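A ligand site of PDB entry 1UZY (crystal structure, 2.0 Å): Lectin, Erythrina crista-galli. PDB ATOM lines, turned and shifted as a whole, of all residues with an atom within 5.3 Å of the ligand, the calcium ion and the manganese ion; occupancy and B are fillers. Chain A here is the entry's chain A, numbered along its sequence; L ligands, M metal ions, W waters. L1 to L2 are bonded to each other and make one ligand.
ND2 of Asn 133 sits at hydrogen-bond distance from O2 of LG2 L2 (2.9 Å).
OD1 of Asp 89 sits at hydrogen-bond distance from O3 of LG2 L2, 2.6 Å away.
O3 of LG2 L2 lies within hydrogen-bond range of N of Ala 218.
An oxygen (O2) of LG2 L2 is in hydrogen-bond range of the backbone NH (N) of Gly 107 (3.1 Å).
The side-chain amide nitrogen (NE2) of Gln 219 sits at hydrogen-bond distance from an oxygen (O3) of LIG L1, at 3.1 Å.
The side-chain carboxylate (OD2) of Asp 89 sits at hydrogen-bond distance from the backbone NH (N) of Gly 107, at 3.3 Å.
The backbone NH (N) of Gly 217 sits at hydrogen-bond distance from the backbone carbonyl oxygen (O) of Ala 222 (2.7 Å).
Ala 88 touches the ligand.
Tyr 106 touches the ligand.
CA of Gly 217 touches O3 of LG2 L2, at 3.1 Å.
Ala 222 touches the ligand.
Hydrophobic or aromatic side chains within 4 Å of the ligand: Ala 88, Tyr 106, Phe 131, Ala 218 and Ala 222.
The nearest printed residue that does not touch the ligand is Leu 86 (4.6 Å).
Four residues have an atom within 4 Å of the calcium ion: Asp 129, Phe 131, Asn 133 and Asp 136.
The nearest printed residue that does not touch the calcium ion is Trp 135 (4.5 Å).
Four residues have an atom within 4 Å of the manganese ion: Glu 127, Asp 129, Asp 136 and His 142.
The calcium ion is bound by OD1 of Asn 133, OD2 of Asp 136, O of Phe 131, OD2 of Asp 129, water W7, water W10 and OD1 of Asp 129.
The calcium ion has seven donor atoms within binding distance.
The manganese ion is bound by the side-chain carboxylate (OD2) of Asp 129 (2.1 Å), the side-chain carboxylate (OE2) of Glu 127 (2.2 Å), the side-chain carboxylate (OD1) of Asp 136 (2.2 Å), water W11 (2.2 Å), water W9 (2.3 Å) and a ring nitrogen (NE2) of His 142 (2.4 Å).
The manganese ion has six donor atoms within binding distance.
Water W7 bridges the backbone carbonyl oxygen of Gly 107 and the indole nitrogen of Trp 135.
Water W9 bridges the side-chain carboxylate of Glu 127 (2.6 Å) and the backbone carbonyl oxygen of Ile 150 (2.7 Å).
Water W12 lies within hydrogen-bond range of an oxygen (O5) of LG2 L2 (2.6 Å) and the backbone carbonyl oxygen (O) of Leu 86 (2.7 Å).
Water W13 lies within hydrogen-bond range of ND2 of Asn 133 and O1 of LG2 L2.
Water W1 lies within hydrogen-bond range of the backbone carbonyl oxygen (O) of Ala 218 and an oxygen (O2) of LIG L1.
Water W5 lies within hydrogen-bond range of the backbone NH (N) of Gly 107, an oxygen (O1) of LG2 L2 and the side-chain amide nitrogen (ND2) of Asn 133.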
ATOM      1  N   PRO A  85     -19.372  -0.722 -11.379  1.00  0.00           N
ATOM      2  CA  PRO A  85     -18.611  -1.245 -12.517  1.00  0.00           C
ATOM      3  C   PRO A  85     -17.589  -0.184 -12.901  1.00  0.00           C
ATOM      4  O   PRO A  85     -17.285   0.695 -12.098  1.00  0.00           O
ATOM      5  CB  PRO A  85     -19.684  -1.427 -13.570  1.00  0.00           C
ATOM      6  CG  PRO A  85     -20.560  -0.243 -13.328  1.00  0.00           C
ATOM      7  CD  PRO A  85     -20.690  -0.231 -11.814  1.00  0.00           C
ATOM      8  N   LEU A  86     -17.070  -0.244 -14.122  1.00  0.00           N
ATOM      9  CA  LEU A  86     -16.088   0.748 -14.568  1.00  0.00           C
ATOM     10  C   LEU A  86     -16.754   2.131 -14.655  1.00  0.00           C
ATOM     11  O   LEU A  86     -17.916   2.246 -15.039  1.00  0.00           O
ATOM     12  CB  LEU A  86     -15.521   0.364 -15.931  1.00  0.00           C
ATOM     13  CG  LEU A  86     -14.684  -0.923 -15.973  1.00  0.00           C
ATOM     14  CD1 LEU A  86     -14.333  -1.248 -17.411  1.00  0.00           C
ATOM     15  CD2 LEU A  86     -13.430  -0.754 -15.133  1.00  0.00           C
ATOM     16  N   ALA A  88     -17.540   6.080 -15.970  1.00  0.00           N
ATOM     17  CA  ALA A  88     -17.807   6.648 -17.297  1.00  0.00           C
ATOM     18  C   ALA A  88     -18.527   7.987 -17.126  1.00  0.00           C
ATOM     19  O   ALA A  88     -19.050   8.254 -16.034  1.00  0.00           O
ATOM     20  CB  ALA A  88     -18.684   5.680 -18.102  1.00  0.00           C
ATOM     21  N   ASP A  89     -18.561   8.838 -18.147  1.00  0.00           N
ATOM     22  CA  ASP A  89     -17.941   8.627 -19.457  1.00  0.00           C
ATOM     23  C   ASP A  89     -16.882   9.694 -19.744  1.00  0.00           C
ATOM     24  O   ASP A  89     -15.994   9.483 -20.570  1.00  0.00           O
ATOM     25  CB  ASP A  89     -18.979   8.686 -20.576  1.00  0.00           C
ATOM     26  CG  ASP A  89     -19.570   7.326 -20.905  1.00  0.00           C
ATOM     27  OD1 ASP A  89     -20.672   7.034 -20.406  1.00  0.00           O
ATOM     28  OD2 ASP A  89     -18.915   6.563 -21.655  1.00  0.00           O
ATOM     29  N   TYR A 106     -23.668   9.416 -22.631  1.00  0.00           N
ATOM     30  CA  TYR A 106     -22.721   8.314 -22.516  1.00  0.00           C
ATOM     31  C   TYR A 106     -21.417   8.667 -23.237  1.00  0.00           C
ATOM     32  O   TYR A 106     -20.890   9.762 -23.046  1.00  0.00           O
ATOM     33  CB  TYR A 106     -23.340   7.028 -23.084  1.00  0.00           C
ATOM     34  CG  TYR A 106     -24.686   6.692 -22.468  1.00  0.00           C
ATOM     35  CD1 TYR A 106     -25.652   5.979 -23.192  1.00  0.00           C
ATOM     36  CD2 TYR A 106     -25.020   7.120 -21.173  1.00  0.00           C
ATOM     37  CE1 TYR A 106     -26.908   5.699 -22.644  1.00  0.00           C
ATOM     38  CE2 TYR A 106     -26.275   6.841 -20.624  1.00  0.00           C
ATOM     39  CZ  TYR A 106     -27.213   6.139 -21.371  1.00  0.00           C
ATOM     40  OH  TYR A 106     -28.470   5.877 -20.851  1.00  0.00           O
ATOM     41  N   GLY A 107     -20.917   7.755 -24.057  1.00  0.00           N
ATOM     42  CA  GLY A 107     -19.674   7.970 -24.781  1.00  0.00           C
ATOM     43  C   GLY A 107     -19.656   9.133 -25.763  1.00  0.00           C
ATOM     44  O   GLY A 107     -18.583   9.540 -26.204  1.00  0.00           O
ATOM     45  N   GLU A 127     -11.541  16.315 -25.581  1.00  0.00           N
ATOM     46  CA  GLU A 127     -12.145  15.450 -24.587  1.00  0.00           C
ATOM     47  C   GLU A 127     -11.200  14.906 -23.525  1.00  0.00           C
ATOM     48  O   GLU A 127      -9.989  14.765 -23.744  1.00  0.00           O
ATOM     49  CB  GLU A 127     -12.806  14.251 -25.288  1.00  0.00           C
ATOM     50  CG  GLU A 127     -11.802  13.405 -26.083  1.00  0.00           C
ATOM     51  CD  GLU A 127     -12.397  12.107 -26.574  1.00  0.00           C
ATOM     52  OE1 GLU A 127     -13.427  12.151 -27.276  1.00  0.00           O
ATOM     53  OE2 GLU A 127     -11.829  11.037 -26.264  1.00  0.00           O
ATOM     54  N   ASP A 129     -11.709  11.781 -21.699  1.00  0.00           N
ATOM     55  CA  ASP A 129     -12.455  10.538 -21.759  1.00  0.00           C
ATOM     56  C   ASP A 129     -12.094   9.466 -20.725  1.00  0.00           C
ATOM     57  O   ASP A 129     -10.959   8.997 -20.691  1.00  0.00           O
ATOM     58  CB  ASP A 129     -12.251  10.006 -23.176  1.00  0.00           C
ATOM     59  CG  ASP A 129     -13.255   8.971 -23.550  1.00  0.00           C
ATOM     60  OD1 ASP A 129     -13.869   8.395 -22.627  1.00  0.00           O
ATOM     61  OD2 ASP A 129     -13.416   8.731 -24.766  1.00  0.00           O
ATOM     62  N   PHE A 131     -14.012   6.344 -20.164  1.00  0.00           N
ATOM     63  CA  PHE A 131     -14.463   4.977 -20.456  1.00  0.00           C
ATOM     64  C   PHE A 131     -14.061   4.600 -21.868  1.00  0.00           C
ATOM     65  O   PHE A 131     -14.272   5.360 -22.796  1.00  0.00           O
ATOM     66  CB  PHE A 131     -15.991   4.882 -20.349  1.00  0.00           C
ATOM     67  CG  PHE A 131     -16.535   3.510 -20.630  1.00  0.00           C
ATOM     68  CD1 PHE A 131     -16.624   2.556 -19.617  1.00  0.00           C
ATOM     69  CD2 PHE A 131     -16.913   3.156 -21.921  1.00  0.00           C
ATOM     70  CE1 PHE A 131     -17.094   1.271 -19.888  1.00  0.00           C
ATOM     71  CE2 PHE A 131     -17.379   1.864 -22.199  1.00  0.00           C
ATOM     72  CZ  PHE A 131     -17.468   0.927 -21.186  1.00  0.00           C
ATOM     73  N   SER A 132     -13.513   3.401 -22.060  1.00  0.00           N
ATOM     74  CA  SER A 132     -13.108   3.007 -23.401  1.00  0.00           C
ATOM     75  C   SER A 132     -14.230   2.369 -24.224  1.00  0.00           C
ATOM     76  O   SER A 132     -14.598   1.217 -23.997  1.00  0.00           O
ATOM     77  CB  SER A 132     -11.921   2.030 -23.319  1.00  0.00           C
ATOM     78  OG  SER A 132     -11.464   1.688 -24.606  1.00  0.00           O
ATOM     79  N   ASN A 133     -14.768   3.125 -25.178  1.00  0.00           N
ATOM     80  CA  ASN A 133     -15.830   2.626 -26.054  1.00  0.00           C
ATOM     81  C   ASN A 133     -15.166   1.907 -27.237  1.00  0.00           C
ATOM     82  O   ASN A 133     -13.944   1.946 -27.400  1.00  0.00           O
ATOM     83  CB  ASN A 133     -16.706   3.772 -26.583  1.00  0.00           C
ATOM     84  CG  ASN A 133     -17.488   4.462 -25.480  1.00  0.00           C
ATOM     85  OD1 ASN A 133     -17.018   5.437 -24.904  1.00  0.00           O
ATOM     86  ND2 ASN A 133     -18.683   3.973 -25.189  1.00  0.00           N
ATOM     87  N   TRP A 135     -14.866   2.644 -30.262  1.00  0.00           N
ATOM     88  CA  TRP A 135     -14.130   3.555 -31.142  1.00  0.00           C
ATOM     89  C   TRP A 135     -12.928   4.191 -30.443  1.00  0.00           C
ATOM     90  O   TRP A 135     -12.217   4.982 -31.060  1.00  0.00           O
ATOM     91  CB  TRP A 135     -15.061   4.661 -31.626  1.00  0.00           C
ATOM     92  CG  TRP A 135     -15.681   5.437 -30.481  1.00  0.00           C
ATOM     93  CD1 TRP A 135     -15.097   6.418 -29.740  1.00  0.00           C
ATOM     94  CD2 TRP A 135     -17.002   5.250 -29.944  1.00  0.00           C
ATOM     95  NE1 TRP A 135     -15.965   6.854 -28.767  1.00  0.00           N
ATOM     96  CE2 TRP A 135     -17.147   6.162 -28.872  1.00  0.00           C
ATOM     97  CE3 TRP A 135     -18.081   4.413 -30.266  1.00  0.00           C
ATOM     98  CZ2 TRP A 135     -18.308   6.252 -28.117  1.00  0.00           C
ATOM     99  CZ3 TRP A 135     -19.250   4.497 -29.511  1.00  0.00           C
ATOM    100  CH2 TRP A 135     -19.355   5.420 -28.454  1.00  0.00           C
ATOM    101  N   ASP A 136     -12.719   3.860 -29.170  1.00  0.00           N
ATOM    102  CA  ASP A 136     -11.624   4.428 -28.374  1.00  0.00           C
ATOM    103  C   ASP A 136     -10.377   3.579 -28.253  1.00  0.00           C
ATOM    104  O   ASP A 136     -10.400   2.371 -28.495  1.00  0.00           O
ATOM    105  CB  ASP A 136     -12.061   4.633 -26.910  1.00  0.00           C
ATOM    106  CG  ASP A 136     -12.932   5.839 -26.711  1.00  0.00           C
ATOM    107  OD1 ASP A 136     -12.650   6.898 -27.294  1.00  0.00           O
ATOM    108  OD2 ASP A 136     -13.894   5.698 -25.943  1.00  0.00           O
ATOM    109  N   PRO A 137      -9.264   4.215 -27.861  1.00  0.00           N
ATOM    110  CA  PRO A 137      -8.030   3.457 -27.683  1.00  0.00           C
ATOM    111  C   PRO A 137      -8.362   2.714 -26.383  1.00  0.00           C
ATOM    112  O   PRO A 137      -9.282   3.120 -25.662  1.00  0.00           O
ATOM    113  CB  PRO A 137      -6.976   4.549 -27.495  1.00  0.00           C
ATOM    114  CG  PRO A 137      -7.747   5.693 -26.904  1.00  0.00           C
ATOM    115  CD  PRO A 137      -9.001   5.663 -27.758  1.00  0.00           C
ATOM    116  N   HIS A 142      -8.058   9.285 -21.175  1.00  0.00           N
ATOM    117  CA  HIS A 142      -7.214   9.801 -22.236  1.00  0.00           C
ATOM    118  C   HIS A 142      -7.760  11.125 -22.725  1.00  0.00           C
ATOM    119  O   HIS A 142      -8.982  11.374 -22.682  1.00  0.00           O
ATOM    120  CB  HIS A 142      -7.107   8.815 -23.419  1.00  0.00           C
ATOM    121  CG  HIS A 142      -8.415   8.491 -24.079  1.00  0.00           C
ATOM    122  ND1 HIS A 142      -9.102   7.323 -23.838  1.00  0.00           N
ATOM    123  CD2 HIS A 142      -9.149   9.178 -24.996  1.00  0.00           C
ATOM    124  CE1 HIS A 142     -10.203   7.292 -24.572  1.00  0.00           C
ATOM    125  NE2 HIS A 142     -10.254   8.416 -25.281  1.00  0.00           N
ATOM    126  N   ILE A 150     -16.552  11.646 -32.678  1.00  0.00           N
ATOM    127  CA  ILE A 150     -16.161  11.233 -31.343  1.00  0.00           C
ATOM    128  C   ILE A 150     -14.914  10.348 -31.483  1.00  0.00           C
ATOM    129  O   ILE A 150     -14.253  10.013 -30.500  1.00  0.00           O
ATOM    130  CB  ILE A 150     -17.282  10.440 -30.643  1.00  0.00           C
ATOM    131  CG1 ILE A 150     -16.944  10.236 -29.172  1.00  0.00           C
ATOM    132  CG2 ILE A 150     -17.507   9.105 -31.357  1.00  0.00           C
ATOM    133  CD1 ILE A 150     -16.906  11.532 -28.357  1.00  0.00           C
ATOM    134  N   SER A 152     -11.585  10.384 -32.057  1.00  0.00           N
ATOM    135  CA  SER A 152     -10.474  11.331 -31.999  1.00  0.00           C
ATOM    136  C   SER A 152      -9.422  11.182 -33.095  1.00  0.00           C
ATOM    137  O   SER A 152      -9.029  10.070 -33.450  1.00  0.00           O
ATOM    138  CB  SER A 152      -9.761  11.210 -30.637  1.00  0.00           C
ATOM    139  OG  SER A 152     -10.687  11.301 -29.568  1.00  0.00           O
ATOM    140  N   THR A 155      -5.083  11.020 -29.603  1.00  0.00           N
ATOM    141  CA  THR A 155      -5.369  10.796 -28.187  1.00  0.00           C
ATOM    142  C   THR A 155      -4.082  10.687 -27.383  1.00  0.00           C
ATOM    143  O   THR A 155      -3.017  10.367 -27.921  1.00  0.00           O
ATOM    144  CB  THR A 155      -6.199   9.502 -27.945  1.00  0.00           C
ATOM    145  OG1 THR A 155      -5.481   8.370 -28.435  1.00  0.00           O
ATOM    146  CG2 THR A 155      -7.568   9.594 -28.639  1.00  0.00           C
ATOM    147  N   THR A 216     -22.319  10.813 -17.560  1.00  0.00           N
ATOM    148  CA  THR A 216     -22.049   9.590 -16.797  1.00  0.00           C
ATOM    149  C   THR A 216     -22.598   8.430 -17.638  1.00  0.00           C
ATOM    150  O   THR A 216     -23.238   8.661 -18.678  1.00  0.00           O
ATOM    151  CB  THR A 216     -22.678   9.611 -15.394  1.00  0.00           C
ATOM    152  OG1 THR A 216     -24.057   9.988 -15.480  1.00  0.00           O
ATOM    153  CG2 THR A 216     -21.928  10.591 -14.498  1.00  0.00           C
ATOM    154  N   GLY A 217     -22.327   7.200 -17.186  1.00  0.00           N
ATOM    155  CA  GLY A 217     -22.649   5.935 -17.882  1.00  0.00           C
ATOM    156  C   GLY A 217     -24.096   5.458 -18.088  1.00  0.00           C
ATOM    157  O   GLY A 217     -25.062   6.002 -17.571  1.00  0.00           O
ATOM    158  N   ALA A 218     -24.154   4.381 -18.910  1.00  0.00           N
ATOM    159  CA  ALA A 218     -25.375   3.705 -19.325  1.00  0.00           C
ATOM    160  C   ALA A 218     -25.903   2.586 -18.432  1.00  0.00           C
ATOM    161  O   ALA A 218     -26.913   1.944 -18.779  1.00  0.00           O
ATOM    162  CB  ALA A 218     -25.191   3.168 -20.747  1.00  0.00           C
ATOM    163  N   GLN A 219     -25.232   2.315 -17.316  1.00  0.00           N
ATOM    164  CA  GLN A 219     -25.672   1.299 -16.379  1.00  0.00           C
ATOM    165  C   GLN A 219     -25.418   1.788 -14.955  1.00  0.00           C
ATOM    166  O   GLN A 219     -24.540   2.627 -14.723  1.00  0.00           O
ATOM    167  CB  GLN A 219     -24.971  -0.051 -16.605  1.00  0.00           C
ATOM    168  CG  GLN A 219     -23.476  -0.076 -16.342  1.00  0.00           C
ATOM    169  CD  GLN A 219     -22.921  -1.471 -16.455  1.00  0.00           C
ATOM    170  OE1 GLN A 219     -22.665  -2.133 -15.446  1.00  0.00           O
ATOM    171  NE2 GLN A 219     -22.728  -1.939 -17.680  1.00  0.00           N
ATOM    172  N   ALA A 222     -22.100   3.300 -13.155  1.00  0.00           N
ATOM    173  CA  ALA A 222     -21.024   3.561 -14.127  1.00  0.00           C
ATOM    174  C   ALA A 222     -21.030   5.085 -14.181  1.00  0.00           C
ATOM    175  O   ALA A 222     -21.537   5.691 -15.123  1.00  0.00           O
ATOM    176  CB  ALA A 222     -21.304   2.940 -15.485  1.00  0.00           C
HETATM  177  C1  LIG L   1     -24.663  -2.056 -20.945  1.00  0.00           C
HETATM  178  C2  LIG L   1     -24.425  -0.556 -21.117  1.00  0.00           C
HETATM  179  C3  LIG L   1     -23.534  -0.330 -22.349  1.00  0.00           C
HETATM  180  C4  LIG L   1     -24.250  -0.931 -23.601  1.00  0.00           C
HETATM  181  C5  LIG L   1     -23.409  -0.790 -24.859  1.00  0.00           C
HETATM  182  C6  LIG L   1     -25.364  -2.593 -22.212  1.00  0.00           C
HETATM  183  O1  LIG L   1     -25.578  -3.954 -22.084  1.00  0.00           O
HETATM  184  O2  LIG L   1     -25.503  -2.277 -19.814  1.00  0.00           O
HETATM  185  O3  LIG L   1     -23.771  -0.048 -19.960  1.00  0.00           O
HETATM  186  O4  LIG L   1     -23.301   1.089 -22.541  1.00  0.00           O
HETATM  187  O5  LIG L   1     -24.522  -2.360 -23.392  1.00  0.00           O
HETATM  188  O6  LIG L   1     -24.119  -1.252 -25.999  1.00  0.00           O
HETATM  189  C1  LG2 L   2     -22.050   1.614 -22.170  1.00  0.00           C
HETATM  190  C2  LG2 L   2     -21.900   3.014 -22.805  1.00  0.00           C
HETATM  191  C3  LG2 L   2     -20.533   3.619 -22.411  1.00  0.00           C
HETATM  192  C4  LG2 L   2     -20.440   3.734 -20.866  1.00  0.00           C
HETATM  193  C5  LG2 L   2     -20.647   2.288 -20.306  1.00  0.00           C
HETATM  194  C6  LG2 L   2     -20.603   2.138 -18.821  1.00  0.00           C
HETATM  195  O1  LG2 L   2     -21.992   2.888 -24.216  1.00  0.00           O
HETATM  196  O2  LG2 L   2     -20.394   4.898 -22.995  1.00  0.00           O
HETATM  197  O3  LG2 L   2     -21.463   4.602 -20.389  1.00  0.00           O
HETATM  198  O4  LG2 L   2     -21.926   1.746 -20.747  1.00  0.00           O
HETATM  199  O5  LG2 L   2     -20.820   0.778 -18.487  1.00  0.00           O
HETATM  200 CA    CA M   1     -15.226   7.016 -24.356  1.00  0.00          CA
HETATM  201 MN    MN M   2     -12.202   8.913 -26.529  1.00  0.00          MN
HETATM  202  O   HOH W   1     -27.684  -0.600 -19.215  1.00  0.00           O
HETATM  203  O   HOH W   2     -24.708   2.883 -25.136  1.00  0.00           O
HETATM  204  O   HOH W   3     -25.081   1.099 -27.045  1.00  0.00           O
HETATM  205  O   HOH W   4     -21.845  -4.074 -23.611  1.00  0.00           O
HETATM  206  O   HOH W   5     -21.690   5.455 -25.782  1.00  0.00           O
HETATM  207  O   HOH W   6     -20.157  -1.362 -20.019  1.00  0.00           O
HETATM  208  O   HOH W   7     -16.124   8.614 -26.118  1.00  0.00           O
HETATM  209  O   HOH W   8     -26.199  -3.035 -25.867  1.00  0.00           O
HETATM  210  O   HOH W   9     -13.974   9.681 -27.822  1.00  0.00           O
HETATM  211  O   HOH W  10     -16.824   7.824 -22.536  1.00  0.00           O
HETATM  212  O   HOH W  11     -10.950   8.951 -28.351  1.00  0.00           O
HETATM  213  O   HOH W  12     -19.212   0.401 -16.473  1.00  0.00           O
HETATM  214  O   HOH W  13     -19.977   1.664 -25.722  1.00  0.00           O
HETATM  215  O   HOH W  14     -25.644  -4.848 -19.006  1.00  0.00           O
